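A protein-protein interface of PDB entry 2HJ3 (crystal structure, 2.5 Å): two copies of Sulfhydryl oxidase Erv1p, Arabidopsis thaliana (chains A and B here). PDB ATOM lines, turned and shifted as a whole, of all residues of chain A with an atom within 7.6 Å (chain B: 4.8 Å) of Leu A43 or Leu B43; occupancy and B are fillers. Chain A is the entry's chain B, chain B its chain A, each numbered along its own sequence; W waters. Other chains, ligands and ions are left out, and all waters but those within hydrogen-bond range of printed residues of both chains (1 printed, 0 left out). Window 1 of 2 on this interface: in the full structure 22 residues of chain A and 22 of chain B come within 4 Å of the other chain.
Among the printed residues, pairs that only touch across the chains: Met A50 with Leu B24 (3.2 Å), Met A50 with Val B40 (3.3 Å), Met A50 with Asp B39 (3.3 Å), Asp A39 with Ile B46 (3.5 Å), Phe A20 with Leu B47 (3.5 Å), Leu A47 with Phe B20 (3.6 Å), Ile A46 with Glu B42 (3.7 Å), Ile A46 with Asp B39 (3.8 Å), Ile A46 with Ile B46 (3.9 Å), Ile A46 with Leu B43 (3.9 Å), Leu A43 with Ile B46 (3.9 Å), Glu A42 with Glu B42 (3.9 Å), Leu A43 with Leu B43 (3.9 Å) and Met A50 with Leu B43 (3.97 Å).
Phe A20 touches Leu B47, and with the chains exchanged Leu A47 touches Phe B20. Asp A39 touches Ile B46, and with the chains exchanged Ile A46 touches Asp B39. Glu B42 touches its own counterpart, Glu A42. Leu A43 touches Ile B46, and with the chains exchanged Ile A46 touches Leu B43. Positions printed for both chains: 20, 21, 24, 39, 40, 41, 42, 43, 44, 45, 46 and 47.
Water W1 lies within hydrogen-bond range of the side-chain carboxylate (OE2) of Glu A42 (2.7 Å) and the side-chain carboxylate (OD1) of Asp B39 (3.1 Å).
Among the printed residues, 15 pairs touch across the chains. Among the printed residues, Asp or Glu carboxylates within 4 Å of a Lys or Arg side-chain nitrogen of the other chain: Arg A49 with Asp B39 (3.1 Å).
The side-chain carboxylate (OD1) of Asp B39 lies within salt-bridge range of the guanidinium group (NH1) of Arg A49.
Of chain B, only Leu B43 and Ile B46 come within 4 Å of Leu A43. Thr A45 touches none of the printed residues of chain B. Printed residues of chain A within 4 Å of Phe B20: Leu A47. Of the printed residues of chain A, Asp B39 touches Ile A46, Arg A49 and Met A50. Leu B43 touches three residues of chain A. Of the printed residues of chain A, Leu B47 touches Phe A20 (3.5 Å). The nearest printed residue of chain B that does not touch Arg A49 is Leu B24 (7.3 Å).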
ATOM      1  N   PHE A  20      -8.048 -11.124  13.935  1.00  0.00           N
ATOM      2  CA  PHE A  20      -9.305 -11.857  13.919  1.00  0.00           C
ATOM      3  C   PHE A  20      -9.558 -12.490  15.291  1.00  0.00           C
ATOM      4  O   PHE A  20     -10.589 -12.252  15.926  1.00  0.00           O
ATOM      5  CB  PHE A  20      -9.267 -12.947  12.829  1.00  0.00           C
ATOM      6  CG  PHE A  20     -10.333 -13.995  12.983  1.00  0.00           C
ATOM      7  CD1 PHE A  20     -11.677 -13.655  12.912  1.00  0.00           C
ATOM      8  CD2 PHE A  20      -9.994 -15.312  13.260  1.00  0.00           C
ATOM      9  CE1 PHE A  20     -12.673 -14.611  13.119  1.00  0.00           C
ATOM     10  CE2 PHE A  20     -10.986 -16.281  13.470  1.00  0.00           C
ATOM     11  CZ  PHE A  20     -12.326 -15.927  13.402  1.00  0.00           C
ATOM     12  N   LEU A  21      -8.602 -13.293  15.744  1.00  0.00           N
ATOM     13  CA  LEU A  21      -8.717 -13.975  17.027  1.00  0.00           C
ATOM     14  C   LEU A  21      -9.016 -13.040  18.186  1.00  0.00           C
ATOM     15  O   LEU A  21     -10.011 -13.200  18.898  1.00  0.00           O
ATOM     16  CB  LEU A  21      -7.432 -14.753  17.316  1.00  0.00           C
ATOM     17  CG  LEU A  21      -7.154 -15.882  16.328  1.00  0.00           C
ATOM     18  CD1 LEU A  21      -5.818 -16.546  16.641  1.00  0.00           C
ATOM     19  CD2 LEU A  21      -8.292 -16.887  16.398  1.00  0.00           C
ATOM     20  N   LEU A  24     -12.301 -11.511  18.042  1.00  0.00           N
ATOM     21  CA  LEU A  24     -13.278 -12.534  18.379  1.00  0.00           C
ATOM     22  C   LEU A  24     -13.303 -12.690  19.902  1.00  0.00           C
ATOM     23  O   LEU A  24     -14.365 -12.759  20.508  1.00  0.00           O
ATOM     24  CB  LEU A  24     -12.900 -13.863  17.719  1.00  0.00           C
ATOM     25  CG  LEU A  24     -13.794 -15.065  18.040  1.00  0.00           C
ATOM     26  CD1 LEU A  24     -15.065 -14.995  17.214  1.00  0.00           C
ATOM     27  CD2 LEU A  24     -13.064 -16.350  17.734  1.00  0.00           C
ATOM     28  N   GLN A  36     -21.268 -21.926  22.180  1.00  0.00           N
ATOM     29  CA  GLN A  36     -20.229 -20.925  22.000  1.00  0.00           C
ATOM     30  C   GLN A  36     -18.889 -21.377  22.572  1.00  0.00           C
ATOM     31  O   GLN A  36     -17.842 -21.158  21.954  1.00  0.00           O
ATOM     32  CB  GLN A  36     -20.674 -19.611  22.632  1.00  0.00           C
ATOM     33  CG  GLN A  36     -21.937 -19.064  21.977  1.00  0.00           C
ATOM     34  CD  GLN A  36     -22.473 -17.818  22.643  1.00  0.00           C
ATOM     35  OE1 GLN A  36     -22.693 -17.835  23.877  1.00  0.00           O
ATOM     36  NE2 GLN A  36     -22.684 -16.820  21.924  1.00  0.00           N
ATOM     37  N   LYS A  37     -18.917 -22.016  23.741  1.00  0.00           N
ATOM     38  CA  LYS A  37     -17.692 -22.503  24.360  1.00  0.00           C
ATOM     39  C   LYS A  37     -17.121 -23.560  23.438  1.00  0.00           C
ATOM     40  O   LYS A  37     -15.928 -23.548  23.110  1.00  0.00           O
ATOM     41  CB  LYS A  37     -17.975 -23.139  25.723  1.00  0.00           C
ATOM     42  CG  LYS A  37     -18.624 -22.210  26.727  1.00  0.00           C
ATOM     43  CD  LYS A  37     -18.653 -22.824  28.116  1.00  0.00           C
ATOM     44  CE  LYS A  37     -19.467 -21.956  29.076  1.00  0.00           C
ATOM     45  NZ  LYS A  37     -19.546 -22.510  30.464  1.00  0.00           N
ATOM     46  N   LYS A  38     -17.988 -24.475  23.017  1.00  0.00           N
ATOM     47  CA  LYS A  38     -17.584 -25.556  22.133  1.00  0.00           C
ATOM     48  C   LYS A  38     -17.003 -25.051  20.803  1.00  0.00           C
ATOM     49  O   LYS A  38     -15.986 -25.562  20.328  1.00  0.00           O
ATOM     50  CB  LYS A  38     -18.777 -26.481  21.862  1.00  0.00           C
ATOM     51  CG  LYS A  38     -18.450 -27.640  20.932  1.00  0.00           C
ATOM     52  CD  LYS A  38     -19.680 -28.465  20.605  1.00  0.00           C
ATOM     53  CE  LYS A  38     -19.326 -29.596  19.656  1.00  0.00           C
ATOM     54  NZ  LYS A  38     -20.477 -30.511  19.397  1.00  0.00           N
ATOM     55  N   ASP A  39     -17.646 -24.056  20.205  1.00  0.00           N
ATOM     56  CA  ASP A  39     -17.173 -23.516  18.934  1.00  0.00           C
ATOM     57  C   ASP A  39     -15.828 -22.828  19.047  1.00  0.00           C
ATOM     58  O   ASP A  39     -14.964 -23.003  18.186  1.00  0.00           O
ATOM     59  CB  ASP A  39     -18.209 -22.559  18.349  1.00  0.00           C
ATOM     60  CG  ASP A  39     -19.408 -23.292  17.768  1.00  0.00           C
ATOM     61  OD1 ASP A  39     -19.372 -24.541  17.731  1.00  0.00           O
ATOM     62  OD2 ASP A  39     -20.372 -22.624  17.344  1.00  0.00           O
ATOM     63  N   VAL A  40     -15.645 -22.056  20.114  1.00  0.00           N
ATOM     64  CA  VAL A  40     -14.384 -21.364  20.345  1.00  0.00           C
ATOM     65  C   VAL A  40     -13.256 -22.369  20.527  1.00  0.00           C
ATOM     66  O   VAL A  40     -12.153 -22.196  19.996  1.00  0.00           O
ATOM     67  CB  VAL A  40     -14.477 -20.461  21.588  1.00  0.00           C
ATOM     68  CG1 VAL A  40     -13.124 -20.341  22.253  1.00  0.00           C
ATOM     69  CG2 VAL A  40     -14.957 -19.091  21.177  1.00  0.00           C
ATOM     70  N   LYS A  41     -13.527 -23.429  21.276  1.00  0.00           N
ATOM     71  CA  LYS A  41     -12.512 -24.448  21.494  1.00  0.00           C
ATOM     72  C   LYS A  41     -12.179 -25.182  20.210  1.00  0.00           C
ATOM     73  O   LYS A  41     -11.007 -25.370  19.881  1.00  0.00           O
ATOM     74  CB  LYS A  41     -12.977 -25.456  22.538  1.00  0.00           C
ATOM     75  CG  LYS A  41     -13.058 -24.910  23.946  1.00  0.00           C
ATOM     76  CD  LYS A  41     -13.484 -26.019  24.887  1.00  0.00           C
ATOM     77  CE  LYS A  41     -13.560 -25.538  26.319  1.00  0.00           C
ATOM     78  NZ  LYS A  41     -14.067 -26.619  27.212  1.00  0.00           N
ATOM     79  N   GLU A  42     -13.208 -25.609  19.485  1.00  0.00           N
ATOM     80  CA  GLU A  42     -12.994 -26.334  18.234  1.00  0.00           C
ATOM     81  C   GLU A  42     -12.283 -25.409  17.248  1.00  0.00           C
ATOM     82  O   GLU A  42     -11.492 -25.851  16.414  1.00  0.00           O
ATOM     83  CB  GLU A  42     -14.332 -26.800  17.662  1.00  0.00           C
ATOM     84  CG  GLU A  42     -14.235 -27.522  16.329  1.00  0.00           C
ATOM     85  CD  GLU A  42     -13.532 -28.875  16.412  1.00  0.00           C
ATOM     86  OE1 GLU A  42     -13.367 -29.416  17.532  1.00  0.00           O
ATOM     87  OE2 GLU A  42     -13.158 -29.409  15.347  1.00  0.00           O
ATOM     88  N   LEU A  43     -12.552 -24.117  17.361  1.00  0.00           N
ATOM     89  CA  LEU A  43     -11.905 -23.160  16.489  1.00  0.00           C
ATOM     90  C   LEU A  43     -10.389 -23.189  16.666  1.00  0.00           C
ATOM     91  O   LEU A  43      -9.647 -23.130  15.685  1.00  0.00           O
ATOM     92  CB  LEU A  43     -12.416 -21.752  16.764  1.00  0.00           C
ATOM     93  CG  LEU A  43     -11.532 -20.683  16.124  1.00  0.00           C
ATOM     94  CD1 LEU A  43     -11.512 -20.901  14.630  1.00  0.00           C
ATOM     95  CD2 LEU A  43     -12.048 -19.296  16.471  1.00  0.00           C
ATOM     96  N   MET A  44      -9.918 -23.279  17.907  1.00  0.00           N
ATOM     97  CA  MET A  44      -8.477 -23.302  18.128  1.00  0.00           C
ATOM     98  C   MET A  44      -7.910 -24.613  17.612  1.00  0.00           C
ATOM     99  O   MET A  44      -6.843 -24.634  16.999  1.00  0.00           O
ATOM    100  CB  MET A  44      -8.121 -23.124  19.610  1.00  0.00           C
ATOM    101  CG  MET A  44      -8.669 -21.864  20.284  1.00  0.00           C
ATOM    102  SD  MET A  44      -8.515 -20.304  19.374  1.00  0.00           S
ATOM    103  CE  MET A  44      -6.779 -20.164  19.250  1.00  0.00           C
ATOM    104  N   THR A  45      -8.619 -25.711  17.853  1.00  0.00           N
ATOM    105  CA  THR A  45      -8.164 -27.012  17.370  1.00  0.00           C
ATOM    106  C   THR A  45      -8.046 -26.990  15.851  1.00  0.00           C
ATOM    107  O   THR A  45      -7.067 -27.466  15.293  1.00  0.00           O
ATOM    108  CB  THR A  45      -9.144 -28.136  17.755  1.00  0.00           C
ATOM    109  OG1 THR A  45      -9.179 -28.274  19.180  1.00  0.00           O
ATOM    110  CG2 THR A  45      -8.711 -29.454  17.141  1.00  0.00           C
ATOM    111  N   ILE A  46      -9.050 -26.446  15.176  1.00  0.00           N
ATOM    112  CA  ILE A  46      -9.010 -26.383  13.719  1.00  0.00           C
ATOM    113  C   ILE A  46      -7.784 -25.602  13.267  1.00  0.00           C
ATOM    114  O   ILE A  46      -7.107 -25.987  12.312  1.00  0.00           O
ATOM    115  CB  ILE A  46     -10.292 -25.733  13.156  1.00  0.00           C
ATOM    116  CG1 ILE A  46     -11.466 -26.710  13.299  1.00  0.00           C
ATOM    117  CG2 ILE A  46     -10.098 -25.350  11.704  1.00  0.00           C
ATOM    118  CD1 ILE A  46     -12.832 -26.064  13.100  1.00  0.00           C
ATOM    119  N   LEU A  47      -7.488 -24.515  13.973  1.00  0.00           N
ATOM    120  CA  LEU A  47      -6.339 -23.680  13.643  1.00  0.00           C
ATOM    121  C   LEU A  47      -5.013 -24.411  13.771  1.00  0.00           C
ATOM    122  O   LEU A  47      -4.143 -24.269  12.923  1.00  0.00           O
ATOM    123  CB  LEU A  47      -6.317 -22.437  14.533  1.00  0.00           C
ATOM    124  CG  LEU A  47      -7.333 -21.350  14.182  1.00  0.00           C
ATOM    125  CD1 LEU A  47      -7.398 -20.298  15.281  1.00  0.00           C
ATOM    126  CD2 LEU A  47      -6.936 -20.716  12.865  1.00  0.00           C
ATOM    127  N   SER A  48      -4.851 -25.202  14.824  1.00  0.00           N
ATOM    128  CA  SER A  48      -3.594 -25.916  15.014  1.00  0.00           C
ATOM    129  C   SER A  48      -3.321 -26.969  13.942  1.00  0.00           C
ATOM    130  O   SER A  48      -2.189 -27.426  13.791  1.00  0.00           O
ATOM    131  CB  SER A  48      -3.547 -26.564  16.407  1.00  0.00           C
ATOM    132  OG  SER A  48      -4.511 -27.588  16.538  1.00  0.00           O
ATOM    133  N   ARG A  49      -4.347 -27.371  13.202  1.00  0.00           N
ATOM    134  CA  ARG A  49      -4.153 -28.363  12.146  1.00  0.00           C
ATOM    135  C   ARG A  49      -4.038 -27.682  10.796  1.00  0.00           C
ATOM    136  O   ARG A  49      -3.207 -28.039   9.963  1.00  0.00           O
ATOM    137  CB  ARG A  49      -5.350 -29.311  12.047  1.00  0.00           C
ATOM    138  CG  ARG A  49      -5.596 -30.214  13.219  1.00  0.00           C
ATOM    139  CD  ARG A  49      -6.842 -31.032  12.966  1.00  0.00           C
ATOM    140  NE  ARG A  49      -7.269 -31.716  14.179  1.00  0.00           N
ATOM    141  CZ  ARG A  49      -8.535 -31.867  14.539  1.00  0.00           C
ATOM    142  NH1 ARG A  49      -9.503 -31.385  13.775  1.00  0.00           N
ATOM    143  NH2 ARG A  49      -8.827 -32.475  15.679  1.00  0.00           N
ATOM    144  N   MET A  50      -4.899 -26.687  10.621  1.00  0.00           N
ATOM    145  CA  MET A  50      -5.067 -25.939   9.388  1.00  0.00           C
ATOM    146  C   MET A  50      -4.258 -24.664   9.137  1.00  0.00           C
ATOM    147  O   MET A  50      -4.197 -24.199   7.999  1.00  0.00           O
ATOM    148  CB  MET A  50      -6.557 -25.633   9.272  1.00  0.00           C
ATOM    149  CG  MET A  50      -7.045 -25.118   7.956  1.00  0.00           C
ATOM    150  SD  MET A  50      -8.832 -24.900   8.086  1.00  0.00           S
ATOM    151  CE  MET A  50      -9.408 -26.586   7.773  1.00  0.00           C
ATOM    152  N   PHE A  60       1.964 -24.101  17.309  1.00  0.00           N
ATOM    153  CA  PHE A  60       0.716 -23.763  17.971  1.00  0.00           C
ATOM    154  C   PHE A  60       0.044 -25.009  18.545  1.00  0.00           C
ATOM    155  O   PHE A  60      -0.607 -24.945  19.581  1.00  0.00           O
ATOM    156  CB  PHE A  60      -0.231 -23.062  16.985  1.00  0.00           C
ATOM    157  CG  PHE A  60      -1.464 -22.482  17.634  1.00  0.00           C
ATOM    158  CD1 PHE A  60      -1.365 -21.409  18.519  1.00  0.00           C
ATOM    159  CD2 PHE A  60      -2.720 -23.028  17.389  1.00  0.00           C
ATOM    160  CE1 PHE A  60      -2.494 -20.893  19.150  1.00  0.00           C
ATOM    161  CE2 PHE A  60      -3.855 -22.517  18.019  1.00  0.00           C
ATOM    162  CZ  PHE A  60      -3.739 -21.449  18.899  1.00  0.00           C
ATOM    163  N   LEU A  64      -1.188 -25.519  22.432  1.00  0.00           N
ATOM    164  CA  LEU A  64      -2.572 -25.838  22.754  1.00  0.00           C
ATOM    165  C   LEU A  64      -2.628 -27.140  23.562  1.00  0.00           C
ATOM    166  O   LEU A  64      -3.558 -27.358  24.337  1.00  0.00           O
ATOM    167  CB  LEU A  64      -3.385 -25.955  21.463  1.00  0.00           C
ATOM    168  CG  LEU A  64      -4.911 -25.922  21.556  1.00  0.00           C
ATOM    169  CD1 LEU A  64      -5.381 -24.560  22.043  1.00  0.00           C
ATOM    170  CD2 LEU A  64      -5.498 -26.223  20.179  1.00  0.00           C
ATOM    171  N   PHE A  77     -11.243 -16.089  28.250  1.00  0.00           N
ATOM    172  CA  PHE A  77     -10.854 -16.343  26.874  1.00  0.00           C
ATOM    173  C   PHE A  77      -9.866 -15.263  26.406  1.00  0.00           C
ATOM    174  O   PHE A  77      -8.837 -15.575  25.818  1.00  0.00           O
ATOM    175  CB  PHE A  77     -12.101 -16.396  25.979  1.00  0.00           C
ATOM    176  CG  PHE A  77     -11.808 -16.750  24.551  1.00  0.00           C
ATOM    177  CD1 PHE A  77     -10.916 -17.764  24.244  1.00  0.00           C
ATOM    178  CD2 PHE A  77     -12.417 -16.058  23.509  1.00  0.00           C
ATOM    179  CE1 PHE A  77     -10.628 -18.080  22.926  1.00  0.00           C
ATOM    180  CE2 PHE A  77     -12.135 -16.370  22.188  1.00  0.00           C
ATOM    181  CZ  PHE A  77     -11.237 -17.383  21.895  1.00  0.00           C
ATOM    182  N   PHE B  20      -6.838 -14.094   5.952  1.00  0.00           N
ATOM    183  CA  PHE B  20      -6.694 -15.387   6.598  1.00  0.00           C
ATOM    184  C   PHE B  20      -7.454 -16.460   5.806  1.00  0.00           C
ATOM    185  O   PHE B  20      -6.900 -17.507   5.463  1.00  0.00           O
ATOM    186  CB  PHE B  20      -7.222 -15.285   8.038  1.00  0.00           C
ATOM    187  CG  PHE B  20      -7.453 -16.603   8.688  1.00  0.00           C
ATOM    188  CD1 PHE B  20      -6.429 -17.535   8.779  1.00  0.00           C
ATOM    189  CD2 PHE B  20      -8.709 -16.933   9.179  1.00  0.00           C
ATOM    190  CE1 PHE B  20      -6.652 -18.785   9.347  1.00  0.00           C
ATOM    191  CE2 PHE B  20      -8.947 -18.187   9.751  1.00  0.00           C
ATOM    192  CZ  PHE B  20      -7.916 -19.113   9.833  1.00  0.00           C
ATOM    193  N   LEU B  21      -8.724 -16.198   5.509  1.00  0.00           N
ATOM    194  CA  LEU B  21      -9.523 -17.162   4.758  1.00  0.00           C
ATOM    195  C   LEU B  21      -8.981 -17.456   3.353  1.00  0.00           C
ATOM    196  O   LEU B  21      -8.760 -18.614   3.004  1.00  0.00           O
ATOM    197  CB  LEU B  21     -10.981 -16.693   4.689  1.00  0.00           C
ATOM    198  CG  LEU B  21     -11.677 -16.755   6.064  1.00  0.00           C
ATOM    199  CD1 LEU B  21     -13.101 -16.173   5.985  1.00  0.00           C
ATOM    200  CD2 LEU B  21     -11.714 -18.203   6.537  1.00  0.00           C
ATOM    201  N   LEU B  24      -5.804 -19.226   3.471  1.00  0.00           N
ATOM    202  CA  LEU B  24      -6.077 -20.590   3.877  1.00  0.00           C
ATOM    203  C   LEU B  24      -6.537 -21.437   2.691  1.00  0.00           C
ATOM    204  O   LEU B  24      -6.102 -22.579   2.530  1.00  0.00           O
ATOM    205  CB  LEU B  24      -7.140 -20.595   4.967  1.00  0.00           C
ATOM    206  CG  LEU B  24      -7.599 -21.970   5.437  1.00  0.00           C
ATOM    207  CD1 LEU B  24      -6.384 -22.788   5.855  1.00  0.00           C
ATOM    208  CD2 LEU B  24      -8.583 -21.816   6.596  1.00  0.00           C
ATOM    209  N   ASP B  39     -12.766 -30.007   8.775  1.00  0.00           N
ATOM    210  CA  ASP B  39     -12.381 -28.803   9.504  1.00  0.00           C
ATOM    211  C   ASP B  39     -12.759 -27.540   8.750  1.00  0.00           C
ATOM    212  O   ASP B  39     -13.253 -26.581   9.342  1.00  0.00           O
ATOM    213  CB  ASP B  39     -10.879 -28.805   9.799  1.00  0.00           C
ATOM    214  CG  ASP B  39     -10.476 -29.940  10.717  1.00  0.00           C
ATOM    215  OD1 ASP B  39     -11.362 -30.454  11.434  1.00  0.00           O
ATOM    216  OD2 ASP B  39      -9.281 -30.306  10.731  1.00  0.00           O
ATOM    217  N   VAL B  40     -12.527 -27.545   7.442  1.00  0.00           N
ATOM    218  CA  VAL B  40     -12.858 -26.404   6.614  1.00  0.00           C
ATOM    219  C   VAL B  40     -14.343 -26.084   6.720  1.00  0.00           C
ATOM    220  O   VAL B  40     -14.727 -24.930   6.876  1.00  0.00           O
ATOM    221  CB  VAL B  40     -12.493 -26.669   5.136  1.00  0.00           C
ATOM    222  CG1 VAL B  40     -13.315 -25.776   4.219  1.00  0.00           C
ATOM    223  CG2 VAL B  40     -11.032 -26.392   4.921  1.00  0.00           C
ATOM    224  N   LYS B  41     -15.180 -27.107   6.637  1.00  0.00           N
ATOM    225  CA  LYS B  41     -16.613 -26.886   6.736  1.00  0.00           C
ATOM    226  C   LYS B  41     -17.006 -26.447   8.128  1.00  0.00           C
ATOM    227  O   LYS B  41     -17.865 -25.582   8.289  1.00  0.00           O
ATOM    228  CB  LYS B  41     -17.373 -28.152   6.360  1.00  0.00           C
ATOM    229  CG  LYS B  41     -17.122 -28.597   4.937  1.00  0.00           C
ATOM    230  CD  LYS B  41     -17.956 -29.800   4.571  1.00  0.00           C
ATOM    231  CE  LYS B  41     -17.597 -30.292   3.176  1.00  0.00           C
ATOM    232  NZ  LYS B  41     -18.263 -31.589   2.830  1.00  0.00           N
ATOM    233  N   GLU B  42     -16.381 -27.039   9.140  1.00  0.00           N
ATOM    234  CA  GLU B  42     -16.693 -26.678  10.518  1.00  0.00           C
ATOM    235  C   GLU B  42     -16.263 -25.236  10.785  1.00  0.00           C
ATOM    236  O   GLU B  42     -16.944 -24.488  11.492  1.00  0.00           O
ATOM    237  CB  GLU B  42     -15.995 -27.642  11.483  1.00  0.00           C
ATOM    238  CG  GLU B  42     -16.284 -27.400  12.973  1.00  0.00           C
ATOM    239  CD  GLU B  42     -17.779 -27.342  13.309  1.00  0.00           C
ATOM    240  OE1 GLU B  42     -18.568 -28.079  12.677  1.00  0.00           O
ATOM    241  OE2 GLU B  42     -18.162 -26.572  14.221  1.00  0.00           O
ATOM    242  N   LEU B  43     -15.137 -24.848  10.200  1.00  0.00           N
ATOM    243  CA  LEU B  43     -14.617 -23.494  10.351  1.00  0.00           C
ATOM    244  C   LEU B  43     -15.623 -22.471   9.828  1.00  0.00           C
ATOM    245  O   LEU B  43     -15.872 -21.453  10.470  1.00  0.00           O
ATOM    246  CB  LEU B  43     -13.290 -23.357   9.597  1.00  0.00           C
ATOM    247  CG  LEU B  43     -12.727 -21.938   9.453  1.00  0.00           C
ATOM    248  CD1 LEU B  43     -12.451 -21.342  10.825  1.00  0.00           C
ATOM    249  CD2 LEU B  43     -11.457 -21.972   8.626  1.00  0.00           C
ATOM    250  N   MET B  44     -16.212 -22.744   8.669  1.00  0.00           N
ATOM    251  CA  MET B  44     -17.190 -21.817   8.104  1.00  0.00           C
ATOM    252  C   MET B  44     -18.438 -21.735   8.979  1.00  0.00           C
ATOM    253  O   MET B  44     -19.000 -20.658   9.174  1.00  0.00           O
ATOM    254  CB  MET B  44     -17.587 -22.233   6.684  1.00  0.00           C
ATOM    255  CG  MET B  44     -16.439 -22.371   5.709  1.00  0.00           C
ATOM    256  SD  MET B  44     -15.199 -21.070   5.840  1.00  0.00           S
ATOM    257  CE  MET B  44     -16.049 -19.752   5.232  1.00  0.00           C
ATOM    258  N   THR B  45     -18.875 -22.875   9.502  1.00  0.00           N
ATOM    259  CA  THR B  45     -20.050 -22.911  10.375  1.00  0.00           C
ATOM    260  C   THR B  45     -19.770 -22.092  11.622  1.00  0.00           C
ATOM    261  O   THR B  45     -20.598 -21.295  12.052  1.00  0.00           O
ATOM    262  CB  THR B  45     -20.379 -24.341  10.818  1.00  0.00           C
ATOM    263  OG1 THR B  45     -20.672 -25.140   9.666  1.00  0.00           O
ATOM    264  CG2 THR B  45     -21.576 -24.347  11.763  1.00  0.00           C
ATOM    265  N   ILE B  46     -18.597 -22.305  12.207  1.00  0.00           N
ATOM    266  CA  ILE B  46     -18.215 -21.560  13.396  1.00  0.00           C
ATOM    267  C   ILE B  46     -18.238 -20.066  13.088  1.00  0.00           C
ATOM    268  O   ILE B  46     -18.806 -19.286  13.848  1.00  0.00           O
ATOM    269  CB  ILE B  46     -16.820 -22.000  13.904  1.00  0.00           C
ATOM    270  CG1 ILE B  46     -16.903 -23.451  14.405  1.00  0.00           C
ATOM    271  CG2 ILE B  46     -16.338 -21.068  15.015  1.00  0.00           C
ATOM    272  CD1 ILE B  46     -15.604 -24.012  14.905  1.00  0.00           C
ATOM    273  N   LEU B  47     -17.649 -19.665  11.967  1.00  0.00           N
ATOM    274  CA  LEU B  47     -17.657 -18.250  11.582  1.00  0.00           C
ATOM    275  C   LEU B  47     -19.074 -17.708  11.415  1.00  0.00           C
ATOM    276  O   LEU B  47     -19.348 -16.558  11.760  1.00  0.00           O
ATOM    277  CB  LEU B  47     -16.905 -18.027  10.265  1.00  0.00           C
ATOM    278  CG  LEU B  47     -15.380 -18.029  10.279  1.00  0.00           C
ATOM    279  CD1 LEU B  47     -14.870 -17.896   8.859  1.00  0.00           C
ATOM    280  CD2 LEU B  47     -14.864 -16.887  11.128  1.00  0.00           C
HETATM  281  O   HOH W   1     -14.058 -29.703  12.783  1.00  0.00           O
